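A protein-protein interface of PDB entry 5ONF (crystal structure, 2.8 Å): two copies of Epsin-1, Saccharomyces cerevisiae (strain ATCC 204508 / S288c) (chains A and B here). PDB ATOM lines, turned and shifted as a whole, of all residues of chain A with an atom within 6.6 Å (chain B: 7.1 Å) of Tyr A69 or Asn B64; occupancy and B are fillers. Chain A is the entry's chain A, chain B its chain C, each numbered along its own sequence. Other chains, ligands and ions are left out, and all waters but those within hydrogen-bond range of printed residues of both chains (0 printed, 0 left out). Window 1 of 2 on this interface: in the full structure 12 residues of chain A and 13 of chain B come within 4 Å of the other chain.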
ATOM      1  N   ASN A  29       2.539  -8.976   3.919  1.00  0.00           N
ATOM      2  CA  ASN A  29       2.770 -10.130   3.046  1.00  0.00           C
ATOM      3  C   ASN A  29       4.221 -10.626   3.008  1.00  0.00           C
ATOM      4  O   ASN A  29       4.574 -11.391   2.105  1.00  0.00           O
ATOM      5  CB  ASN A  29       2.293  -9.797   1.622  1.00  0.00           C
ATOM      6  CG  ASN A  29       3.259  -8.904   0.862  1.00  0.00           C
ATOM      7  OD1 ASN A  29       3.333  -7.700   1.102  1.00  0.00           O
ATOM      8  ND2 ASN A  29       3.994  -9.495  -0.068  1.00  0.00           N
ATOM      9  N   ARG A  62      -9.046 -10.905   5.708  1.00  0.00           N
ATOM     10  CA  ARG A  62      -7.694 -11.470   5.617  1.00  0.00           C
ATOM     11  C   ARG A  62      -7.678 -12.973   5.775  1.00  0.00           C
ATOM     12  O   ARG A  62      -6.815 -13.637   5.202  1.00  0.00           O
ATOM     13  CB  ARG A  62      -6.805 -10.845   6.698  1.00  0.00           C
ATOM     14  CG  ARG A  62      -5.444 -10.390   6.214  1.00  0.00           C
ATOM     15  CD  ARG A  62      -5.519  -9.135   5.312  1.00  0.00           C
ATOM     16  NE  ARG A  62      -4.209  -8.474   5.234  1.00  0.00           N
ATOM     17  CZ  ARG A  62      -3.790  -7.687   4.235  1.00  0.00           C
ATOM     18  NH1 ARG A  62      -4.559  -7.440   3.181  1.00  0.00           N
ATOM     19  NH2 ARG A  62      -2.564  -7.159   4.276  1.00  0.00           N
ATOM     20  N   ASP A  65      -8.459 -15.268   2.431  1.00  0.00           N
ATOM     21  CA  ASP A  65      -7.535 -14.869   1.384  1.00  0.00           C
ATOM     22  C   ASP A  65      -7.225 -16.107   0.546  1.00  0.00           C
ATOM     23  O   ASP A  65      -7.589 -17.237   0.914  1.00  0.00           O
ATOM     24  CB  ASP A  65      -6.238 -14.290   1.990  1.00  0.00           C
ATOM     25  CG  ASP A  65      -5.784 -12.999   1.321  1.00  0.00           C
ATOM     26  OD1 ASP A  65      -6.028 -12.813   0.095  1.00  0.00           O
ATOM     27  OD2 ASP A  65      -5.173 -12.161   2.036  1.00  0.00           O
ATOM     28  N   LYS A  66      -6.528 -15.885  -0.567  1.00  0.00           N
ATOM     29  CA  LYS A  66      -6.199 -16.947  -1.526  1.00  0.00           C
ATOM     30  C   LYS A  66      -5.189 -17.943  -0.966  1.00  0.00           C
ATOM     31  O   LYS A  66      -4.605 -17.731   0.104  1.00  0.00           O
ATOM     32  CB  LYS A  66      -5.623 -16.357  -2.821  1.00  0.00           C
ATOM     33  CG  LYS A  66      -6.549 -15.415  -3.580  1.00  0.00           C
ATOM     34  CD  LYS A  66      -6.137 -15.237  -5.045  1.00  0.00           C
ATOM     35  CE  LYS A  66      -4.703 -14.752  -5.218  1.00  0.00           C
ATOM     36  NZ  LYS A  66      -4.327 -14.482  -6.638  1.00  0.00           N
ATOM     37  N   GLY A  67      -4.988 -19.026  -1.716  1.00  0.00           N
ATOM     38  CA  GLY A  67      -3.916 -19.979  -1.454  1.00  0.00           C
ATOM     39  C   GLY A  67      -2.551 -19.310  -1.424  1.00  0.00           C
ATOM     40  O   GLY A  67      -1.720 -19.607  -0.564  1.00  0.00           O
ATOM     41  N   LYS A  68      -2.345 -18.384  -2.360  1.00  0.00           N
ATOM     42  CA  LYS A  68      -1.074 -17.666  -2.516  1.00  0.00           C
ATOM     43  C   LYS A  68      -0.680 -16.860  -1.285  1.00  0.00           C
ATOM     44  O   LYS A  68       0.488 -16.843  -0.898  1.00  0.00           O
ATOM     45  CB  LYS A  68      -1.148 -16.712  -3.705  1.00  0.00           C
ATOM     46  CG  LYS A  68      -1.329 -17.393  -5.048  1.00  0.00           C
ATOM     47  CD  LYS A  68      -1.250 -16.357  -6.143  1.00  0.00           C
ATOM     48  CE  LYS A  68      -1.161 -16.972  -7.524  1.00  0.00           C
ATOM     49  NZ  LYS A  68      -0.859 -15.880  -8.489  1.00  0.00           N
ATOM     50  N   TYR A  69      -1.655 -16.180  -0.690  1.00  0.00           N
ATOM     51  CA  TYR A  69      -1.416 -15.337   0.470  1.00  0.00           C
ATOM     52  C   TYR A  69      -1.639 -16.148   1.739  1.00  0.00           C
ATOM     53  O   TYR A  69      -2.663 -16.035   2.408  1.00  0.00           O
ATOM     54  CB  TYR A  69      -2.311 -14.100   0.411  1.00  0.00           C
ATOM     55  CG  TYR A  69      -2.078 -13.252  -0.829  1.00  0.00           C
ATOM     56  CD1 TYR A  69      -1.001 -12.366  -0.898  1.00  0.00           C
ATOM     57  CD2 TYR A  69      -2.923 -13.338  -1.937  1.00  0.00           C
ATOM     58  CE1 TYR A  69      -0.776 -11.587  -2.025  1.00  0.00           C
ATOM     59  CE2 TYR A  69      -2.699 -12.556  -3.069  1.00  0.00           C
ATOM     60  CZ  TYR A  69      -1.624 -11.687  -3.102  1.00  0.00           C
ATOM     61  OH  TYR A  69      -1.377 -10.913  -4.201  1.00  0.00           O
ATOM     62  N   TRP A  70      -0.655 -16.984   2.040  1.00  0.00           N
ATOM     63  CA  TRP A  70      -0.634 -17.801   3.258  1.00  0.00           C
ATOM     64  C   TRP A  70      -0.253 -16.949   4.472  1.00  0.00           C
ATOM     65  O   TRP A  70      -0.708 -17.213   5.590  1.00  0.00           O
ATOM     66  CB  TRP A  70       0.319 -19.015   3.122  1.00  0.00           C
ATOM     67  CG  TRP A  70       1.763 -18.709   2.693  1.00  0.00           C
ATOM     68  CD1 TRP A  70       2.213 -18.489   1.412  1.00  0.00           C
ATOM     69  CD2 TRP A  70       2.929 -18.634   3.535  1.00  0.00           C
ATOM     70  NE1 TRP A  70       3.571 -18.261   1.410  1.00  0.00           N
ATOM     71  CE2 TRP A  70       4.038 -18.346   2.695  1.00  0.00           C
ATOM     72  CE3 TRP A  70       3.145 -18.773   4.917  1.00  0.00           C
ATOM     73  CZ2 TRP A  70       5.345 -18.188   3.193  1.00  0.00           C
ATOM     74  CZ3 TRP A  70       4.452 -18.616   5.415  1.00  0.00           C
ATOM     75  CH2 TRP A  70       5.529 -18.324   4.551  1.00  0.00           C
ATOM     76  N   ARG A  71       0.561 -15.917   4.241  1.00  0.00           N
ATOM     77  CA  ARG A  71       1.116 -15.082   5.318  1.00  0.00           C
ATOM     78  C   ARG A  71       0.087 -14.137   5.915  1.00  0.00           C
ATOM     79  O   ARG A  71       0.107 -13.874   7.124  1.00  0.00           O
ATOM     80  CB  ARG A  71       2.310 -14.271   4.811  1.00  0.00           C
ATOM     81  CG  ARG A  71       3.465 -15.133   4.330  1.00  0.00           C
ATOM     82  CD  ARG A  71       4.548 -14.284   3.712  1.00  0.00           C
ATOM     83  NE  ARG A  71       4.267 -13.965   2.311  1.00  0.00           N
ATOM     84  CZ  ARG A  71       4.883 -14.481   1.240  1.00  0.00           C
ATOM     85  NH1 ARG A  71       5.865 -15.377   1.345  1.00  0.00           N
ATOM     86  NH2 ARG A  71       4.512 -14.085   0.025  1.00  0.00           N
ATOM     87  N   HIS A  72      -0.794 -13.612   5.064  1.00  0.00           N
ATOM     88  CA  HIS A  72      -1.945 -12.851   5.528  1.00  0.00           C
ATOM     89  C   HIS A  72      -2.771 -13.677   6.507  1.00  0.00           C
ATOM     90  O   HIS A  72      -3.120 -13.213   7.580  1.00  0.00           O
ATOM     91  CB  HIS A  72      -2.813 -12.422   4.346  1.00  0.00           C
ATOM     92  CG  HIS A  72      -2.168 -11.401   3.461  1.00  0.00           C
ATOM     93  ND1 HIS A  72      -2.734 -10.974   2.278  1.00  0.00           N
ATOM     94  CD2 HIS A  72      -0.992 -10.741   3.576  1.00  0.00           C
ATOM     95  CE1 HIS A  72      -1.941 -10.083   1.710  1.00  0.00           C
ATOM     96  NE2 HIS A  72      -0.878  -9.924   2.477  1.00  0.00           N
ATOM     97  N   ILE A  73      -3.015 -14.933   6.153  1.00  0.00           N
ATOM     98  CA  ILE A  73      -3.844 -15.835   6.968  1.00  0.00           C
ATOM     99  C   ILE A  73      -3.046 -16.322   8.190  1.00  0.00           C
ATOM    100  O   ILE A  73      -3.627 -16.616   9.252  1.00  0.00           O
ATOM    101  CB  ILE A  73      -4.364 -17.059   6.164  1.00  0.00           C
ATOM    102  CG1 ILE A  73      -4.839 -16.654   4.752  1.00  0.00           C
ATOM    103  CG2 ILE A  73      -5.517 -17.722   6.912  1.00  0.00           C
ATOM    104  CD1 ILE A  73      -5.167 -17.804   3.821  1.00  0.00           C
ATOM    105  N   ALA A  74      -1.723 -16.424   8.022  1.00  0.00           N
ATOM    106  CA  ALA A  74      -0.815 -16.810   9.105  1.00  0.00           C
ATOM    107  C   ALA A  74      -0.779 -15.763  10.198  1.00  0.00           C
ATOM    108  O   ALA A  74      -1.024 -16.074  11.372  1.00  0.00           O
ATOM    109  CB  ALA A  74       0.595 -17.056   8.569  1.00  0.00           C
ATOM    110  N   PHE A 108      -6.081 -26.227   4.702  1.00  0.00           N
ATOM    111  CA  PHE A 108      -5.597 -25.206   3.769  1.00  0.00           C
ATOM    112  C   PHE A 108      -4.443 -25.739   2.923  1.00  0.00           C
ATOM    113  O   PHE A 108      -3.373 -26.073   3.446  1.00  0.00           O
ATOM    114  CB  PHE A 108      -5.146 -23.943   4.516  1.00  0.00           C
ATOM    115  CG  PHE A 108      -4.596 -22.864   3.612  1.00  0.00           C
ATOM    116  CD1 PHE A 108      -5.424 -22.202   2.713  1.00  0.00           C
ATOM    117  CD2 PHE A 108      -3.248 -22.512   3.653  1.00  0.00           C
ATOM    118  CE1 PHE A 108      -4.929 -21.211   1.878  1.00  0.00           C
ATOM    119  CE2 PHE A 108      -2.744 -21.522   2.818  1.00  0.00           C
ATOM    120  CZ  PHE A 108      -3.586 -20.869   1.933  1.00  0.00           C
ATOM    121  N   HIS A 110      -1.626 -25.321   0.030  1.00  0.00           N
ATOM    122  CA  HIS A 110      -0.758 -24.493  -0.795  1.00  0.00           C
ATOM    123  C   HIS A 110       0.681 -25.038  -0.851  1.00  0.00           C
ATOM    124  O   HIS A 110       1.596 -24.480  -0.235  1.00  0.00           O
ATOM    125  CB  HIS A 110      -0.772 -23.044  -0.309  1.00  0.00           C
ATOM    126  CG  HIS A 110      -0.122 -22.099  -1.266  1.00  0.00           C
ATOM    127  ND1 HIS A 110      -0.598 -21.893  -2.542  1.00  0.00           N
ATOM    128  CD2 HIS A 110       0.974 -21.317  -1.140  1.00  0.00           C
ATOM    129  CE1 HIS A 110       0.175 -21.020  -3.162  1.00  0.00           C
ATOM    130  NE2 HIS A 110       1.136 -20.652  -2.331  1.00  0.00           N
ATOM    131  N   VAL A 122      -0.483 -22.393   8.387  1.00  0.00           N
ATOM    132  CA  VAL A 122      -1.858 -21.906   8.379  1.00  0.00           C
ATOM    133  C   VAL A 122      -2.786 -22.934   9.030  1.00  0.00           C
ATOM    134  O   VAL A 122      -3.552 -22.599   9.931  1.00  0.00           O
ATOM    135  CB  VAL A 122      -2.330 -21.597   6.933  1.00  0.00           C
ATOM    136  CG1 VAL A 122      -3.795 -21.160   6.905  1.00  0.00           C
ATOM    137  CG2 VAL A 122      -1.451 -20.521   6.289  1.00  0.00           C
ATOM    138  N   LEU B  59      -6.594  -2.132 -12.235  1.00  0.00           N
ATOM    139  CA  LEU B  59      -5.578  -3.062 -12.722  1.00  0.00           C
ATOM    140  C   LEU B  59      -5.106  -3.943 -11.573  1.00  0.00           C
ATOM    141  O   LEU B  59      -4.913  -5.151 -11.767  1.00  0.00           O
ATOM    142  CB  LEU B  59      -4.407  -2.335 -13.391  1.00  0.00           C
ATOM    143  CG  LEU B  59      -4.751  -1.665 -14.726  1.00  0.00           C
ATOM    144  CD1 LEU B  59      -3.563  -0.882 -15.256  1.00  0.00           C
ATOM    145  CD2 LEU B  59      -5.220  -2.655 -15.778  1.00  0.00           C
ATOM    146  N   ASP B  60      -4.957  -3.364 -10.377  1.00  0.00           N
ATOM    147  CA  ASP B  60      -4.588  -4.154  -9.190  1.00  0.00           C
ATOM    148  C   ASP B  60      -5.708  -5.127  -8.761  1.00  0.00           C
ATOM    149  O   ASP B  60      -5.453  -6.304  -8.484  1.00  0.00           O
ATOM    150  CB  ASP B  60      -4.169  -3.242  -8.026  1.00  0.00           C
ATOM    151  CG  ASP B  60      -3.448  -3.997  -6.906  1.00  0.00           C
ATOM    152  OD1 ASP B  60      -3.111  -5.187  -7.102  1.00  0.00           O
ATOM    153  OD2 ASP B  60      -3.220  -3.395  -5.825  1.00  0.00           O
ATOM    154  N   LYS B  61      -6.948  -4.645  -8.753  1.00  0.00           N
ATOM    155  CA  LYS B  61      -8.112  -5.500  -8.460  1.00  0.00           C
ATOM    156  C   LYS B  61      -8.309  -6.663  -9.470  1.00  0.00           C
ATOM    157  O   LYS B  61      -9.058  -7.614  -9.190  1.00  0.00           O
ATOM    158  CB  LYS B  61      -9.391  -4.659  -8.355  1.00  0.00           C
ATOM    159  CG  LYS B  61      -9.538  -3.936  -7.026  1.00  0.00           C
ATOM    160  CD  LYS B  61     -10.915  -3.306  -6.877  1.00  0.00           C
ATOM    161  CE  LYS B  61     -11.226  -2.944  -5.433  1.00  0.00           C
ATOM    162  NZ  LYS B  61     -10.346  -1.867  -4.912  1.00  0.00           N
ATOM    163  N   ARG B  62      -7.650  -6.570 -10.630  1.00  0.00           N
ATOM    164  CA  ARG B  62      -7.684  -7.608 -11.663  1.00  0.00           C
ATOM    165  C   ARG B  62      -6.448  -8.501 -11.720  1.00  0.00           C
ATOM    166  O   ARG B  62      -6.517  -9.583 -12.296  1.00  0.00           O
ATOM    167  CB  ARG B  62      -7.906  -6.975 -13.049  1.00  0.00           C
ATOM    168  CG  ARG B  62      -9.343  -6.566 -13.330  1.00  0.00           C
ATOM    169  CD  ARG B  62     -10.265  -7.776 -13.283  1.00  0.00           C
ATOM    170  NE  ARG B  62     -11.581  -7.547 -13.864  1.00  0.00           N
ATOM    171  CZ  ARG B  62     -11.832  -7.408 -15.164  1.00  0.00           C
ATOM    172  NH1 ARG B  62     -10.853  -7.432 -16.055  1.00  0.00           N
ATOM    173  NH2 ARG B  62     -13.078  -7.222 -15.587  1.00  0.00           N
ATOM    174  N   LEU B  63      -5.324  -8.052 -11.163  1.00  0.00           N
ATOM    175  CA  LEU B  63      -4.120  -8.889 -11.084  1.00  0.00           C
ATOM    176  C   LEU B  63      -4.214 -10.030 -10.070  1.00  0.00           C
ATOM    177  O   LEU B  63      -3.617 -11.100 -10.276  1.00  0.00           O
ATOM    178  CB  LEU B  63      -2.877  -8.055 -10.773  1.00  0.00           C
ATOM    179  CG  LEU B  63      -2.309  -7.196 -11.898  1.00  0.00           C
ATOM    180  CD1 LEU B  63      -1.046  -6.522 -11.389  1.00  0.00           C
ATOM    181  CD2 LEU B  63      -2.021  -7.981 -13.165  1.00  0.00           C
ATOM    182  N   ASN B  64      -4.955  -9.803  -8.988  1.00  0.00           N
ATOM    183  CA  ASN B  64      -5.195 -10.828  -7.971  1.00  0.00           C
ATOM    184  C   ASN B  64      -6.537 -11.508  -8.229  1.00  0.00           C
ATOM    185  O   ASN B  64      -7.307 -11.773  -7.289  1.00  0.00           O
ATOM    186  CB  ASN B  64      -5.172 -10.204  -6.572  1.00  0.00           C
ATOM    187  CG  ASN B  64      -3.952  -9.334  -6.347  1.00  0.00           C
ATOM    188  OD1 ASN B  64      -2.851  -9.843  -6.156  1.00  0.00           O
ATOM    189  ND2 ASN B  64      -4.141  -8.009  -6.386  1.00  0.00           N
ATOM    190  N   ASP B  65      -6.811 -11.808  -9.499  1.00  0.00           N
ATOM    191  CA  ASP B  65      -8.025 -12.508  -9.877  1.00  0.00           C
ATOM    192  C   ASP B  65      -7.741 -13.987  -9.739  1.00  0.00           C
ATOM    193  O   ASP B  65      -6.579 -14.400  -9.629  1.00  0.00           O
ATOM    194  CB  ASP B  65      -8.424 -12.183 -11.328  1.00  0.00           C
ATOM    195  CG  ASP B  65      -9.928 -12.144 -11.540  1.00  0.00           C
ATOM    196  OD1 ASP B  65     -10.696 -12.635 -10.679  1.00  0.00           O
ATOM    197  OD2 ASP B  65     -10.343 -11.607 -12.594  1.00  0.00           O
ATOM    198  N   LYS B  66      -8.804 -14.779  -9.792  1.00  0.00           N
ATOM    199  CA  LYS B  66      -8.721 -16.221  -9.587  1.00  0.00           C
ATOM    200  C   LYS B  66      -7.984 -16.914 -10.734  1.00  0.00           C
ATOM    201  O   LYS B  66      -7.667 -16.295 -11.762  1.00  0.00           O
ATOM    202  CB  LYS B  66     -10.126 -16.817  -9.471  1.00  0.00           C
ATOM    203  CG  LYS B  66     -10.996 -16.271  -8.341  1.00  0.00           C
ATOM    204  CD  LYS B  66     -12.484 -16.496  -8.618  1.00  0.00           C
ATOM    205  CE  LYS B  66     -12.826 -17.964  -8.859  1.00  0.00           C
ATOM    206  NZ  LYS B  66     -14.278 -18.191  -9.095  1.00  0.00           N
ATOM    207  N   ILE B  73      -5.720 -11.410 -16.093  1.00  0.00           N
ATOM    208  CA  ILE B  73      -4.411 -11.183 -15.484  1.00  0.00           C
ATOM    209  C   ILE B  73      -3.382 -10.889 -16.580  1.00  0.00           C
ATOM    210  O   ILE B  73      -2.469 -10.080 -16.382  1.00  0.00           O
ATOM    211  CB  ILE B  73      -3.941 -12.376 -14.614  1.00  0.00           C
ATOM    212  CG1 ILE B  73      -5.056 -12.851 -13.658  1.00  0.00           C
ATOM    213  CG2 ILE B  73      -2.723 -11.978 -13.784  1.00  0.00           C
ATOM    214  CD1 ILE B  73      -4.744 -14.106 -12.860  1.00  0.00           C
ATOM    215  N   ASN B  98       3.616  -1.631  -5.183  1.00  0.00           N
ATOM    216  CA  ASN B  98       2.883  -2.915  -5.243  1.00  0.00           C
ATOM    217  C   ASN B  98       3.634  -3.921  -6.132  1.00  0.00           C
ATOM    218  O   ASN B  98       3.035  -4.666  -6.923  1.00  0.00           O
ATOM    219  CB  ASN B  98       1.410  -2.754  -5.681  1.00  0.00           C
ATOM    220  CG  ASN B  98       1.248  -2.260  -7.103  1.00  0.00           C
ATOM    221  OD1 ASN B  98       2.136  -1.624  -7.660  1.00  0.00           O
ATOM    222  ND2 ASN B  98       0.099  -2.554  -7.699  1.00  0.00           N
ATOM    223  N   TYR B 100       5.262  -6.452  -4.946  1.00  0.00           N
ATOM    224  CA  TYR B 100       4.915  -7.757  -4.354  1.00  0.00           C
ATOM    225  C   TYR B 100       3.827  -8.549  -5.106  1.00  0.00           C
ATOM    226  O   TYR B 100       3.840  -9.787  -5.083  1.00  0.00           O
ATOM    227  CB  TYR B 100       4.523  -7.595  -2.868  1.00  0.00           C
ATOM    228  CG  TYR B 100       3.155  -6.968  -2.603  1.00  0.00           C
ATOM    229  CD1 TYR B 100       2.058  -7.762  -2.255  1.00  0.00           C
ATOM    230  CD2 TYR B 100       2.961  -5.583  -2.684  1.00  0.00           C
ATOM    231  CE1 TYR B 100       0.812  -7.202  -2.006  1.00  0.00           C
ATOM    232  CE2 TYR B 100       1.715  -5.015  -2.439  1.00  0.00           C
ATOM    233  CZ  TYR B 100       0.645  -5.826  -2.100  1.00  0.00           C
ATOM    234  OH  TYR B 100      -0.587  -5.269  -1.856  1.00  0.00           O
ATOM    235  N   ILE B 101       2.900  -7.833  -5.748  1.00  0.00           N
ATOM    236  CA  ILE B 101       1.843  -8.440  -6.573  1.00  0.00           C
ATOM    237  C   ILE B 101       2.403  -8.823  -7.942  1.00  0.00           C
ATOM    238  O   ILE B 101       1.993  -9.828  -8.518  1.00  0.00           O
ATOM    239  CB  ILE B 101       0.624  -7.491  -6.740  1.00  0.00           C
ATOM    240  CG1 ILE B 101       0.047  -7.124  -5.361  1.00  0.00           C
ATOM    241  CG2 ILE B 101      -0.465  -8.133  -7.599  1.00  0.00           C
ATOM    242  CD1 ILE B 101      -0.761  -5.849  -5.335  1.00  0.00           C
ATOM    243  N   ILE B 102       3.331  -8.014  -8.457  1.00  0.00           N
ATOM    244  CA  ILE B 102       3.995  -8.288  -9.735  1.00  0.00           C
ATOM    245  C   ILE B 102       4.995  -9.441  -9.594  1.00  0.00           C
ATOM    246  O   ILE B 102       5.025 -10.342 -10.435  1.00  0.00           O
ATOM    247  CB  ILE B 102       4.722  -7.035 -10.291  1.00  0.00           C
ATOM    248  CG1 ILE B 102       3.748  -5.853 -10.495  1.00  0.00           C
ATOM    249  CG2 ILE B 102       5.441  -7.357 -11.598  1.00  0.00           C
ATOM    250  CD1 ILE B 102       2.667  -6.061 -11.539  1.00  0.00           C
ATOM    251  N   THR B 104       5.175 -11.929  -7.366  1.00  0.00           N
ATOM    252  CA  THR B 104       4.504 -13.212  -7.125  1.00  0.00           C
ATOM    253  C   THR B 104       3.869 -13.837  -8.385  1.00  0.00           C
ATOM    254  O   THR B 104       3.770 -15.062  -8.480  1.00  0.00           O
ATOM    255  CB  THR B 104       3.472 -13.104  -5.962  1.00  0.00           C
ATOM    256  OG1 THR B 104       3.076 -14.411  -5.530  1.00  0.00           O
ATOM    257  CG2 THR B 104       2.229 -12.310  -6.347  1.00  0.00           C
ATOM    258  N   LEU B 105       3.472 -13.007  -9.352  1.00  0.00           N
ATOM    259  CA  LEU B 105       2.840 -13.500 -10.584  1.00  0.00           C
ATOM    260  C   LEU B 105       3.798 -14.170 -11.576  1.00  0.00           C
ATOM    261  O   LEU B 105       3.338 -14.745 -12.569  1.00  0.00           O
ATOM    262  CB  LEU B 105       2.075 -12.374 -11.290  1.00  0.00           C
ATOM    263  CG  LEU B 105       0.797 -11.903 -10.589  1.00  0.00           C
ATOM    264  CD1 LEU B 105       0.300 -10.607 -11.204  1.00  0.00           C
ATOM    265  CD2 LEU B 105      -0.300 -12.952 -10.640  1.00  0.00           C
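OH of Tyr A69 is in hydrogen-bond range of OD1 of Asn B64 (2.7 Å).
The backbone carbonyl oxygen (O) of Asn A29 lies within hydrogen-bond range of the guanidinium group (NE) of Arg A71, at 2.6 Å. The side-chain amide nitrogen (ND2) of Asn B64 lies within hydrogen-bond range of the backbone carbonyl oxygen (O) of Asp B60.
Tyr B100 touches Asn A29 (CD1 to ND2, 3.4 Å). Lys A66 touches Asn B64. Lys A66 touches Asp B65. Lys A68 touches Leu B105 (NZ to CD2, 3.7 Å).
Of the printed residues of chain B, Asn A29 touches Tyr B100 (3.4 Å). Of chain B, only Asn B64 (2.7 Å) comes within 4 Å of Tyr A69. Ala A74 touches none of the printed residues of chain B. Printed residues of chain A within 4 Å of Asp B65: Lys A66. Printed residues of chain A within 4 Å of Tyr B100: Asn A29 (3.4 Å). Ile B102 touches none of the printed residues of chain A. The nearest residue of chain B that does not touch Tyr A69 is Ile B101 (4.2 Å).
Of the 15 printed residues of chain A, 4 touch a printed residue of chain B. Printed residues of chain A that touch a printed residue of chain B: Asn A29, Lys A66, Lys A68 and Tyr A69. Along chain A the printed residues that touch a printed residue of chain B span positions 29 to 69. Of the 15 printed residues of chain B, 4 touch a printed residue of chain A. Printed residues of chain B that touch a printed residue of chain A: Asn B64, Asp B65, Tyr B100 and Leu B105.
Lys A66 touches Asp B65, but with the chains exchanged Asp A65 does not touch Lys B66 (9.7 Å). Positions printed for both chains: 62, 65, 66 and 73.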
